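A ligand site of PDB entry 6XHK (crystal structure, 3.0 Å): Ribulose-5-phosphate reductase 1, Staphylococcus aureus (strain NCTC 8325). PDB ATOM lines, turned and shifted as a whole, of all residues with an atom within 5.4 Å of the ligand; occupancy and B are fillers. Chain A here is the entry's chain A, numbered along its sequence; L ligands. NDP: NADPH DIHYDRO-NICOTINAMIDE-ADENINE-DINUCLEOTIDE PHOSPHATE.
The side-chain carboxylate of Asp 172 lies within hydrogen-bond range of an oxygen (O3B) of the ligand (2.6 Å).
The side-chain amino group (NZ) of Lys 201 is in salt-bridge range of an oxygen (O2X) of the ligand, at 3.3 Å.
N of Asn 174 sits at hydrogen-bond distance from O1N of the ligand, at 3.1 Å.
The side-chain amide nitrogen (ND2) of Asn 174 sits at hydrogen-bond distance from an oxygen (O2N) of the ligand, at 3.5 Å.
An oxygen (O1N) of the ligand is in hydrogen-bond range of the backbone NH (N) of Leu 175 (3.2 Å).
The backbone NH of Val 257 is in hydrogen-bond range of an oxygen (O3D) of the ligand (3.3 Å).
O of Val 257 lies within hydrogen-bond range of O3D of the ligand (3.3 Å).
N7N of the ligand lies within hydrogen-bond range of O of Ser 279.
NZ of Lys 197 is in salt-bridge range of O1X of the ligand (3.9 Å).
N7N of the ligand is in hydrogen-bond range of O of Leu 255 (3.4 Å).
The backbone carbonyl oxygen (O) of Gly 234 sits at hydrogen-bond distance from a nitrogen (N6A) of the ligand, 3.4 Å away.
N of Arg 281 lies within hydrogen-bond range of O7N of the ligand (3.5 Å).
An oxygen (O7N) of the ligand lies close to the backbone carbonyl oxygen (O) of Ser 280 (3.2 Å).
CZ of CME 38 touches O2N of the ligand, 3.1 Å away.
Arg 43 touches the ligand.
Val 148 touches the ligand (CG1 to C7N, 3.6 Å).
Trp 170 touches the ligand (CD1 to N1A, 3.8 Å).
Gly 171 touches the ligand (CA to N3A, 3.4 Å).
CA of Gly 173 touches O2A of the ligand (3.4 Å).
Phe 195 touches the ligand.
CG2 of Ile 214 touches N1A of the ligand, 3.7 Å away.
Cys 229 touches the ligand.
CG2 of Val 230 touches N3A of the ligand, at 3.4 Å.
CA of Gly 231 touches O3D of the ligand (3.4 Å).
CB of Ser 237 touches N6A of the ligand, at 3.7 Å.
N of Ala 238 touches N6A of the ligand (3.98 Å).
Gly 256 touches the ligand (CA to O4D, 3.98 Å).
Within 4 Å of the ligand: CME 38, Arg 43, Val 148, Trp 170, Gly 171, Asp 172, Gly 173, Asn 174, Leu 175, Phe 195, Lys 197, Lys 201, Ile 214, Cys 229, Val 230, Gly 231, Gly 234, Ser 237, Ala 238, Leu 255, Gly 256, Val 257, Ser 279, Ser 280 and Arg 281.
The nearest printed residue that does not touch the ligand is Leu 145 (4.001 Å).
OD2 of Asp 172 is in hydrogen-bond range of N of Lys 197, at 2.9 Å.
The backbone NH (N) of Thr 198 is in hydrogen-bond range of the side-chain carboxylate (OD2) of Asp 172, 3.2 Å away.
OH of CME 38 sits at hydrogen-bond distance from the side-chain amide nitrogen of Asn 174 (3.4 Å).
The backbone carbonyl oxygen (O) of Val 257 lies within hydrogen-bond range of the backbone NH (N) of Gly 232 (3.0 Å).
The backbone carbonyl oxygen (O) of Phe 195 lies within hydrogen-bond range of the backbone NH (N) of Gly 171, at 2.8 Å.
N of Ile 214 lies within hydrogen-bond range of O of Gly 196 (3.0 Å).
The backbone carbonyl oxygen of Ile 214 is in hydrogen-bond range of the side-chain amide nitrogen of Gln 241 (3.0 Å).
NE1 of Trp 170 sits at hydrogen-bond distance from OE1 of Gln 241 (2.7 Å).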
ATOM      1  N   CME A  38      19.273 -27.410  38.275  1.00  0.00           N
ATOM      2  CA  CME A  38      18.246 -26.775  37.455  1.00  0.00           C
ATOM      3  CB  CME A  38      17.723 -25.449  38.040  1.00  0.00           C
ATOM      4  SG  CME A  38      16.102 -24.914  37.599  1.00  0.00           S
ATOM      5  SD  CME A  38      14.980 -26.686  37.329  1.00  0.00           S
ATOM      6  CE  CME A  38      14.775 -26.887  35.598  1.00  0.00           C
ATOM      7  CZ  CME A  38      14.178 -28.213  35.176  1.00  0.00           C
ATOM      8  OH  CME A  38      15.100 -29.254  35.458  1.00  0.00           O
ATOM      9  C   CME A  38      18.839 -26.497  36.074  1.00  0.00           C
ATOM     10  O   CME A  38      20.041 -26.286  35.855  1.00  0.00           O
ATOM     11  N   ALA A  39      17.935 -26.497  35.088  1.00  0.00           N
ATOM     12  CA  ALA A  39      18.217 -26.044  33.731  1.00  0.00           C
ATOM     13  C   ALA A  39      18.919 -24.677  33.758  1.00  0.00           C
ATOM     14  O   ALA A  39      19.890 -24.433  33.039  1.00  0.00           O
ATOM     15  CB  ALA A  39      16.925 -25.948  32.963  1.00  0.00           C
ATOM     16  N   ARG A  43      22.712 -23.465  32.269  1.00  0.00           N
ATOM     17  CA  ARG A  43      23.029 -22.346  31.377  1.00  0.00           C
ATOM     18  C   ARG A  43      24.362 -21.703  31.766  1.00  0.00           C
ATOM     19  O   ARG A  43      25.219 -21.462  30.915  1.00  0.00           O
ATOM     20  CB  ARG A  43      21.890 -21.304  31.384  1.00  0.00           C
ATOM     21  CG  ARG A  43      20.502 -21.856  31.007  1.00  0.00           C
ATOM     22  CD  ARG A  43      19.479 -20.802  30.519  1.00  0.00           C
ATOM     23  NE  ARG A  43      18.581 -20.288  31.569  1.00  0.00           N
ATOM     24  CZ  ARG A  43      17.329 -20.711  31.788  1.00  0.00           C
ATOM     25  NH1 ARG A  43      16.805 -21.701  31.059  1.00  0.00           N
ATOM     26  NH2 ARG A  43      16.594 -20.174  32.766  1.00  0.00           N
ATOM     27  N   GLU A  65      17.577 -25.364  44.185  1.00  0.00           N
ATOM     28  CA  GLU A  65      16.602 -26.362  44.607  1.00  0.00           C
ATOM     29  C   GLU A  65      17.246 -27.249  45.677  1.00  0.00           C
ATOM     30  O   GLU A  65      18.182 -27.998  45.377  1.00  0.00           O
ATOM     31  CB  GLU A  65      16.181 -27.233  43.419  1.00  0.00           C
ATOM     32  CG  GLU A  65      15.421 -26.503  42.354  1.00  0.00           C
ATOM     33  CD  GLU A  65      14.973 -27.402  41.224  1.00  0.00           C
ATOM     34  OE1 GLU A  65      15.357 -28.590  41.211  1.00  0.00           O
ATOM     35  OE2 GLU A  65      14.266 -26.899  40.323  1.00  0.00           O
ATOM     36  N   GLU A 144      11.035 -27.233  44.504  1.00  0.00           N
ATOM     37  CA  GLU A 144      10.793 -25.992  43.756  1.00  0.00           C
ATOM     38  C   GLU A 144       9.979 -26.242  42.493  1.00  0.00           C
ATOM     39  O   GLU A 144       9.107 -25.442  42.137  1.00  0.00           O
ATOM     40  CB  GLU A 144      12.084 -25.294  43.375  1.00  0.00           C
ATOM     41  CG  GLU A 144      11.842 -23.841  43.022  1.00  0.00           C
ATOM     42  CD  GLU A 144      12.797 -23.307  41.977  1.00  0.00           C
ATOM     43  OE1 GLU A 144      13.203 -24.088  41.084  1.00  0.00           O
ATOM     44  OE2 GLU A 144      13.153 -22.100  42.049  1.00  0.00           O
ATOM     45  N   LEU A 145      10.280 -27.320  41.758  1.00  0.00           N
ATOM     46  CA  LEU A 145       9.479 -27.599  40.580  1.00  0.00           C
ATOM     47  C   LEU A 145       8.041 -27.870  40.952  1.00  0.00           C
ATOM     48  O   LEU A 145       7.110 -27.413  40.262  1.00  0.00           O
ATOM     49  CB  LEU A 145      10.059 -28.760  39.787  1.00  0.00           C
ATOM     50  CG  LEU A 145      10.833 -28.301  38.556  1.00  0.00           C
ATOM     51  CD1 LEU A 145      11.861 -27.252  38.910  1.00  0.00           C
ATOM     52  CD2 LEU A 145      11.500 -29.466  37.863  1.00  0.00           C
ATOM     53  N   VAL A 148       6.438 -24.447  41.556  1.00  0.00           N
ATOM     54  CA  VAL A 148       6.177 -23.748  40.288  1.00  0.00           C
ATOM     55  C   VAL A 148       4.899 -24.270  39.666  1.00  0.00           C
ATOM     56  O   VAL A 148       4.006 -23.503  39.244  1.00  0.00           O
ATOM     57  CB  VAL A 148       7.382 -23.915  39.346  1.00  0.00           C
ATOM     58  CG1 VAL A 148       7.039 -23.466  37.964  1.00  0.00           C
ATOM     59  CG2 VAL A 148       8.565 -23.132  39.871  1.00  0.00           C
ATOM     60  N   TRP A 170       1.244 -29.821  27.529  1.00  0.00           N
ATOM     61  CA  TRP A 170       2.290 -29.974  26.524  1.00  0.00           C
ATOM     62  C   TRP A 170       3.658 -30.070  27.204  1.00  0.00           C
ATOM     63  O   TRP A 170       3.962 -29.302  28.119  1.00  0.00           O
ATOM     64  CB  TRP A 170       2.311 -28.818  25.510  1.00  0.00           C
ATOM     65  CG  TRP A 170       1.525 -29.070  24.249  1.00  0.00           C
ATOM     66  CD1 TRP A 170       2.022 -29.245  22.981  1.00  0.00           C
ATOM     67  CD2 TRP A 170       0.105 -29.164  24.137  1.00  0.00           C
ATOM     68  NE1 TRP A 170       0.982 -29.462  22.089  1.00  0.00           N
ATOM     69  CE2 TRP A 170      -0.199 -29.415  22.783  1.00  0.00           C
ATOM     70  CE3 TRP A 170      -0.951 -29.075  25.066  1.00  0.00           C
ATOM     71  CZ2 TRP A 170      -1.492 -29.567  22.330  1.00  0.00           C
ATOM     72  CZ3 TRP A 170      -2.237 -29.240  24.610  1.00  0.00           C
ATOM     73  CH2 TRP A 170      -2.504 -29.473  23.251  1.00  0.00           C
ATOM     74  N   GLY A 171       4.476 -31.023  26.730  1.00  0.00           N
ATOM     75  CA  GLY A 171       5.782 -31.292  27.317  1.00  0.00           C
ATOM     76  C   GLY A 171       5.830 -32.552  28.177  1.00  0.00           C
ATOM     77  O   GLY A 171       5.165 -32.613  29.221  1.00  0.00           O
ATOM     78  N   ASP A 172       6.614 -33.542  27.741  1.00  0.00           N
ATOM     79  CA  ASP A 172       6.733 -34.850  28.392  1.00  0.00           C
ATOM     80  C   ASP A 172       7.932 -34.913  29.342  1.00  0.00           C
ATOM     81  O   ASP A 172       8.547 -35.976  29.492  1.00  0.00           O
ATOM     82  CB  ASP A 172       6.839 -35.932  27.319  1.00  0.00           C
ATOM     83  CG  ASP A 172       7.880 -35.624  26.253  1.00  0.00           C
ATOM     84  OD1 ASP A 172       8.582 -34.616  26.381  1.00  0.00           O
ATOM     85  OD2 ASP A 172       8.039 -36.409  25.306  1.00  0.00           O
ATOM     86  N   GLY A 173       8.308 -33.807  29.992  1.00  0.00           N
ATOM     87  CA  GLY A 173       9.475 -33.746  30.849  1.00  0.00           C
ATOM     88  C   GLY A 173       9.196 -33.547  32.337  1.00  0.00           C
ATOM     89  O   GLY A 173       8.159 -34.010  32.825  1.00  0.00           O
ATOM     90  N   ASN A 174      10.079 -32.862  33.070  1.00  0.00           N
ATOM     91  CA  ASN A 174       9.925 -32.790  34.522  1.00  0.00           C
ATOM     92  C   ASN A 174       8.690 -31.980  34.916  1.00  0.00           C
ATOM     93  O   ASN A 174       7.862 -32.451  35.712  1.00  0.00           O
ATOM     94  CB  ASN A 174      11.180 -32.248  35.211  1.00  0.00           C
ATOM     95  CG  ASN A 174      12.473 -32.899  34.714  1.00  0.00           C
ATOM     96  OD1 ASN A 174      12.513 -34.108  34.442  1.00  0.00           O
ATOM     97  ND2 ASN A 174      13.528 -32.115  34.624  1.00  0.00           N
ATOM     98  N   LEU A 175       8.542 -30.756  34.377  1.00  0.00           N
ATOM     99  CA  LEU A 175       7.332 -29.966  34.664  1.00  0.00           C
ATOM    100  C   LEU A 175       6.060 -30.635  34.157  1.00  0.00           C
ATOM    101  O   LEU A 175       5.037 -30.634  34.862  1.00  0.00           O
ATOM    102  CB  LEU A 175       7.438 -28.579  34.079  1.00  0.00           C
ATOM    103  CG  LEU A 175       7.783 -27.512  35.078  1.00  0.00           C
ATOM    104  CD1 LEU A 175       8.032 -26.191  34.368  1.00  0.00           C
ATOM    105  CD2 LEU A 175       6.573 -27.415  35.990  1.00  0.00           C
ATOM    106  N   GLY A 176       6.084 -31.162  32.933  1.00  0.00           N
ATOM    107  CA  GLY A 176       4.963 -31.983  32.500  1.00  0.00           C
ATOM    108  C   GLY A 176       4.535 -32.987  33.551  1.00  0.00           C
ATOM    109  O   GLY A 176       3.362 -33.013  33.951  1.00  0.00           O
ATOM    110  N   PHE A 195       0.812 -34.275  25.911  1.00  0.00           N
ATOM    111  CA  PHE A 195       1.337 -34.220  24.556  1.00  0.00           C
ATOM    112  C   PHE A 195       2.857 -34.088  24.611  1.00  0.00           C
ATOM    113  O   PHE A 195       3.366 -33.193  25.294  1.00  0.00           O
ATOM    114  CB  PHE A 195       0.736 -33.046  23.762  1.00  0.00           C
ATOM    115  CG  PHE A 195      -0.773 -33.050  23.736  1.00  0.00           C
ATOM    116  CD1 PHE A 195      -1.501 -32.596  24.823  1.00  0.00           C
ATOM    117  CD2 PHE A 195      -1.455 -33.576  22.640  1.00  0.00           C
ATOM    118  CE1 PHE A 195      -2.878 -32.630  24.819  1.00  0.00           C
ATOM    119  CE2 PHE A 195      -2.812 -33.617  22.642  1.00  0.00           C
ATOM    120  CZ  PHE A 195      -3.532 -33.151  23.732  1.00  0.00           C
ATOM    121  N   GLY A 196       3.548 -34.966  23.900  1.00  0.00           N
ATOM    122  CA  GLY A 196       4.997 -34.911  23.937  1.00  0.00           C
ATOM    123  C   GLY A 196       5.621 -35.379  22.657  1.00  0.00           C
ATOM    124  O   GLY A 196       4.943 -35.418  21.629  1.00  0.00           O
ATOM    125  N   LYS A 197       6.887 -35.766  22.715  1.00  0.00           N
ATOM    126  CA  LYS A 197       7.675 -36.108  21.528  1.00  0.00           C
ATOM    127  C   LYS A 197       8.270 -37.526  21.509  1.00  0.00           C
ATOM    128  O   LYS A 197       8.567 -38.022  20.411  1.00  0.00           O
ATOM    129  CB  LYS A 197       8.835 -35.121  21.347  1.00  0.00           C
ATOM    130  CG  LYS A 197       8.441 -33.703  20.964  1.00  0.00           C
ATOM    131  CD  LYS A 197       9.661 -32.800  20.808  1.00  0.00           C
ATOM    132  CE  LYS A 197      10.507 -33.156  19.576  1.00  0.00           C
ATOM    133  NZ  LYS A 197      11.404 -32.067  19.081  1.00  0.00           N
ATOM    134  N   THR A 198       8.477 -38.193  22.648  1.00  0.00           N
ATOM    135  CA  THR A 198       9.265 -39.429  22.693  1.00  0.00           C
ATOM    136  C   THR A 198       8.538 -40.512  23.484  1.00  0.00           C
ATOM    137  O   THR A 198       8.005 -40.241  24.560  1.00  0.00           O
ATOM    138  CB  THR A 198      10.649 -39.195  23.315  1.00  0.00           C
ATOM    139  OG1 THR A 198      10.536 -38.249  24.381  1.00  0.00           O
ATOM    140  CG2 THR A 198      11.611 -38.674  22.267  1.00  0.00           C
ATOM    141  N   LYS A 201       9.743 -40.862  27.258  1.00  0.00           N
ATOM    142  CA  LYS A 201       9.260 -39.946  28.273  1.00  0.00           C
ATOM    143  C   LYS A 201       7.764 -40.092  28.511  1.00  0.00           C
ATOM    144  O   LYS A 201       7.311 -40.046  29.666  1.00  0.00           O
ATOM    145  CB  LYS A 201       9.608 -38.502  27.916  1.00  0.00           C
ATOM    146  CG  LYS A 201      11.099 -38.215  27.891  1.00  0.00           C
ATOM    147  CD  LYS A 201      11.440 -36.811  27.462  1.00  0.00           C
ATOM    148  CE  LYS A 201      12.935 -36.693  27.307  1.00  0.00           C
ATOM    149  NZ  LYS A 201      13.422 -35.369  26.922  1.00  0.00           N
ATOM    150  N   ILE A 214       2.858 -35.095  19.465  1.00  0.00           N
ATOM    151  CA  ILE A 214       2.485 -33.834  18.816  1.00  0.00           C
ATOM    152  C   ILE A 214       2.363 -34.053  17.323  1.00  0.00           C
ATOM    153  O   ILE A 214       1.792 -33.228  16.606  1.00  0.00           O
ATOM    154  CB  ILE A 214       3.511 -32.725  19.180  1.00  0.00           C
ATOM    155  CG1 ILE A 214       4.940 -33.113  18.769  1.00  0.00           C
ATOM    156  CG2 ILE A 214       3.489 -32.455  20.671  1.00  0.00           C
ATOM    157  CD1 ILE A 214       5.900 -31.993  18.830  1.00  0.00           C
ATOM    158  N   CYS A 229       4.377 -26.589  29.374  1.00  0.00           N
ATOM    159  CA  CYS A 229       5.527 -27.013  30.163  1.00  0.00           C
ATOM    160  C   CYS A 229       6.699 -27.398  29.268  1.00  0.00           C
ATOM    161  O   CYS A 229       7.447 -28.352  29.529  1.00  0.00           O
ATOM    162  CB  CYS A 229       5.155 -28.162  31.087  1.00  0.00           C
ATOM    163  SG  CYS A 229       3.717 -27.877  32.091  1.00  0.00           S
ATOM    164  N   VAL A 230       6.818 -26.663  28.159  1.00  0.00           N
ATOM    165  CA  VAL A 230       7.878 -26.746  27.156  1.00  0.00           C
ATOM    166  C   VAL A 230       8.601 -25.411  27.143  1.00  0.00           C
ATOM    167  O   VAL A 230       7.980 -24.365  27.319  1.00  0.00           O
ATOM    168  CB  VAL A 230       7.259 -27.038  25.771  1.00  0.00           C
ATOM    169  CG1 VAL A 230       8.295 -27.128  24.676  1.00  0.00           C
ATOM    170  CG2 VAL A 230       6.398 -28.239  25.826  1.00  0.00           C
ATOM    171  N   GLY A 231       9.916 -25.410  26.943  1.00  0.00           N
ATOM    172  CA  GLY A 231      10.645 -24.177  26.889  1.00  0.00           C
ATOM    173  C   GLY A 231      11.244 -23.897  25.520  1.00  0.00           C
ATOM    174  O   GLY A 231      11.054 -24.622  24.557  1.00  0.00           O
ATOM    175  N   GLY A 232      11.995 -22.796  25.469  1.00  0.00           N
ATOM    176  CA  GLY A 232      12.937 -22.611  24.403  1.00  0.00           C
ATOM    177  C   GLY A 232      12.256 -22.435  23.065  1.00  0.00           C
ATOM    178  O   GLY A 232      11.140 -21.918  22.971  1.00  0.00           O
ATOM    179  N   GLY A 234      10.975 -24.546  21.367  1.00  0.00           N
ATOM    180  CA  GLY A 234       9.821 -25.424  21.286  1.00  0.00           C
ATOM    181  C   GLY A 234       8.536 -24.863  21.844  1.00  0.00           C
ATOM    182  O   GLY A 234       7.448 -25.332  21.469  1.00  0.00           O
ATOM    183  N   SER A 237       6.038 -23.682  19.134  1.00  0.00           N
ATOM    184  CA  SER A 237       5.256 -24.763  18.534  1.00  0.00           C
ATOM    185  C   SER A 237       4.162 -25.238  19.485  1.00  0.00           C
ATOM    186  O   SER A 237       2.996 -25.370  19.092  1.00  0.00           O
ATOM    187  CB  SER A 237       6.202 -25.920  18.199  1.00  0.00           C
ATOM    188  OG  SER A 237       7.461 -25.423  17.752  1.00  0.00           O
ATOM    189  N   ALA A 238       4.540 -25.501  20.726  1.00  0.00           N
ATOM    190  CA  ALA A 238       3.574 -25.954  21.720  1.00  0.00           C
ATOM    191  C   ALA A 238       2.400 -24.990  21.834  1.00  0.00           C
ATOM    192  O   ALA A 238       1.230 -25.412  21.866  1.00  0.00           O
ATOM    193  CB  ALA A 238       4.257 -26.095  23.093  1.00  0.00           C
ATOM    194  N   GLN A 241      -0.004 -24.945  18.792  1.00  0.00           N
ATOM    195  CA  GLN A 241      -0.850 -26.144  18.831  1.00  0.00           C
ATOM    196  C   GLN A 241      -1.969 -26.068  19.858  1.00  0.00           C
ATOM    197  O   GLN A 241      -3.130 -26.368  19.560  1.00  0.00           O
ATOM    198  CB  GLN A 241      -0.024 -27.388  19.065  1.00  0.00           C
ATOM    199  CG  GLN A 241      -0.014 -28.341  17.924  1.00  0.00           C
ATOM    200  CD  GLN A 241       0.807 -29.533  18.220  1.00  0.00           C
ATOM    201  OE1 GLN A 241       1.156 -29.784  19.378  1.00  0.00           O
ATOM    202  NE2 GLN A 241       1.090 -30.328  17.193  1.00  0.00           N
ATOM    203  N   LEU A 255       4.148 -21.770  31.252  1.00  0.00           N
ATOM    204  CA  LEU A 255       5.168 -22.094  32.243  1.00  0.00           C
ATOM    205  C   LEU A 255       6.578 -22.055  31.692  1.00  0.00           C
ATOM    206  O   LEU A 255       7.490 -21.646  32.414  1.00  0.00           O
ATOM    207  CB  LEU A 255       4.905 -23.458  32.867  1.00  0.00           C
ATOM    208  CG  LEU A 255       3.767 -23.378  33.865  1.00  0.00           C
ATOM    209  CD1 LEU A 255       3.410 -24.747  34.387  1.00  0.00           C
ATOM    210  CD2 LEU A 255       4.207 -22.476  35.007  1.00  0.00           C
ATOM    211  N   GLY A 256       6.747 -22.372  30.410  1.00  0.00           N
ATOM    212  CA  GLY A 256       8.061 -22.465  29.812  1.00  0.00           C
ATOM    213  C   GLY A 256       8.715 -21.125  29.530  1.00  0.00           C
ATOM    214  O   GLY A 256       8.079 -20.188  29.028  1.00  0.00           O
ATOM    215  N   VAL A 257       9.995 -21.037  29.836  1.00  0.00           N
ATOM    216  CA  VAL A 257      10.786 -19.845  29.610  1.00  0.00           C
ATOM    217  C   VAL A 257      11.329 -19.868  28.190  1.00  0.00           C
ATOM    218  O   VAL A 257      11.897 -20.880  27.757  1.00  0.00           O
ATOM    219  CB  VAL A 257      11.917 -19.763  30.644  1.00  0.00           C
ATOM    220  CG1 VAL A 257      12.721 -18.500  30.460  1.00  0.00           C
ATOM    221  CG2 VAL A 257      11.312 -19.813  32.041  1.00  0.00           C
ATOM    222  N   SER A 258      11.157 -18.776  27.444  1.00  0.00           N
ATOM    223  CA  SER A 258      11.709 -18.805  26.100  1.00  0.00           C
ATOM    224  C   SER A 258      12.979 -17.980  25.934  1.00  0.00           C
ATOM    225  O   SER A 258      13.714 -18.221  24.972  1.00  0.00           O
ATOM    226  CB  SER A 258      10.678 -18.332  25.076  1.00  0.00           C
ATOM    227  OG  SER A 258      11.339 -18.059  23.851  1.00  0.00           O
ATOM    228  N   SER A 279       2.855 -17.692  34.567  1.00  0.00           N
ATOM    229  CA  SER A 279       3.192 -18.078  35.930  1.00  0.00           C
ATOM    230  C   SER A 279       4.685 -18.396  36.023  1.00  0.00           C
ATOM    231  O   SER A 279       5.212 -19.180  35.227  1.00  0.00           O
ATOM    232  CB  SER A 279       2.378 -19.296  36.379  1.00  0.00           C
ATOM    233  OG  SER A 279       2.750 -19.727  37.672  1.00  0.00           O
ATOM    234  N   SER A 280       5.374 -17.789  37.009  1.00  0.00           N
ATOM    235  CA  SER A 280       6.811 -18.031  37.099  1.00  0.00           C
ATOM    236  C   SER A 280       7.242 -18.450  38.505  1.00  0.00           C
ATOM    237  O   SER A 280       6.825 -19.508  39.018  1.00  0.00           O
ATOM    238  CB  SER A 280       7.585 -16.777  36.659  1.00  0.00           C
ATOM    239  OG  SER A 280       8.938 -17.077  36.374  1.00  0.00           O
ATOM    240  N   ARG A 281       8.101 -17.644  39.133  1.00  0.00           N
ATOM    241  CA  ARG A 281       8.615 -18.002  40.432  1.00  0.00           C
ATOM    242  C   ARG A 281       7.474 -18.080  41.431  1.00  0.00           C
ATOM    243  O   ARG A 281       6.426 -17.436  41.263  1.00  0.00           O
ATOM    244  CB  ARG A 281       9.689 -17.001  40.887  1.00  0.00           C
HETATM  245  PA  NDP L   1      12.742 -30.677  29.843  1.00  0.00           P
HETATM  246  O1A NDP L   1      14.164 -30.818  29.386  1.00  0.00           O
HETATM  247  O2A NDP L   1      12.361 -31.865  30.736  1.00  0.00           O
HETATM  248  O5B NDP L   1      11.757 -30.548  28.510  1.00  0.00           O
HETATM  249  C5B NDP L   1      10.335 -30.883  28.609  1.00  0.00           C
HETATM  250  C4B NDP L   1       9.882 -31.799  27.410  1.00  0.00           C
HETATM  251  O4B NDP L   1       9.244 -31.133  26.473  1.00  0.00           O
HETATM  252  C3B NDP L   1      11.112 -32.433  26.688  1.00  0.00           C
HETATM  253  O3B NDP L   1      11.066 -33.792  26.765  1.00  0.00           O
HETATM  254  C2B NDP L   1      11.000 -32.067  25.209  1.00  0.00           C
HETATM  255  O2B NDP L   1      11.367 -33.321  24.490  1.00  0.00           O
HETATM  256  C1B NDP L   1       9.727 -31.782  25.068  1.00  0.00           C
HETATM  257  N9A NDP L   1       9.404 -30.953  23.901  1.00  0.00           N
HETATM  258  C8A NDP L   1      10.231 -30.330  23.026  1.00  0.00           C
HETATM  259  N7A NDP L   1       9.482 -29.685  22.100  1.00  0.00           N
HETATM  260  C5A NDP L   1       8.211 -29.906  22.389  1.00  0.00           C
HETATM  261  C6A NDP L   1       6.924 -29.442  21.708  1.00  0.00           C
HETATM  262  N6A NDP L   1       7.014 -28.609  20.531  1.00  0.00           N
HETATM  263  N1A NDP L   1       5.669 -29.848  22.247  1.00  0.00           N
HETATM  264  C2A NDP L   1       5.599 -30.689  23.430  1.00  0.00           C
HETATM  265  N3A NDP L   1       6.855 -31.124  24.084  1.00  0.00           N
HETATM  266  C4A NDP L   1       8.156 -30.700  23.510  1.00  0.00           C
HETATM  267  O3  NDP L   1      12.547 -29.288  30.787  1.00  0.00           O
HETATM  268  PN  NDP L   1      11.362 -29.059  31.977  1.00  0.00           P
HETATM  269  O1N NDP L   1      10.209 -30.048  31.794  1.00  0.00           O
HETATM  270  O2N NDP L   1      11.949 -29.319  33.316  1.00  0.00           O
HETATM  271  O5D NDP L   1      10.871 -27.466  31.876  1.00  0.00           O
HETATM  272  C5D NDP L   1      11.081 -26.736  30.655  1.00  0.00           C
HETATM  273  C4D NDP L   1      10.984 -25.285  30.747  1.00  0.00           C
HETATM  274  O4D NDP L   1      10.329 -24.795  32.105  1.00  0.00           O
HETATM  275  C3D NDP L   1      12.354 -24.588  30.702  1.00  0.00           C
HETATM  276  O3D NDP L   1      12.315 -23.417  29.775  1.00  0.00           O
HETATM  277  C2D NDP L   1      12.597 -24.213  31.979  1.00  0.00           C
HETATM  278  O2D NDP L   1      13.526 -23.078  32.111  1.00  0.00           O
HETATM  279  C1D NDP L   1      11.130 -23.870  32.591  1.00  0.00           C
HETATM  280  N1N NDP L   1      11.077 -23.713  34.054  1.00  0.00           N
HETATM  281  C2N NDP L   1      10.202 -22.652  34.578  1.00  0.00           C
HETATM  282  C3N NDP L   1      10.189 -22.227  36.055  1.00  0.00           C
HETATM  283  C7N NDP L   1       9.211 -21.051  36.485  1.00  0.00           C
HETATM  284  O7N NDP L   1       9.439 -20.424  37.487  1.00  0.00           O
HETATM  285  N7N NDP L   1       8.059 -20.746  35.646  1.00  0.00           N
HETATM  286  C4N NDP L   1      10.890 -23.130  37.097  1.00  0.00           C
HETATM  287  C5N NDP L   1      11.939 -24.081  36.471  1.00  0.00           C
HETATM  288  C6N NDP L   1      11.834 -24.539  35.002  1.00  0.00           C
HETATM  289  P2B NDP L   1      12.723 -33.244  23.595  1.00  0.00           P
HETATM  290  O1X NDP L   1      12.745 -31.991  22.740  1.00  0.00           O
HETATM  291  O2X NDP L   1      13.898 -33.192  24.546  1.00  0.00           O
HETATM  292  O3X NDP L   1      12.755 -34.472  22.697  1.00  0.00           O
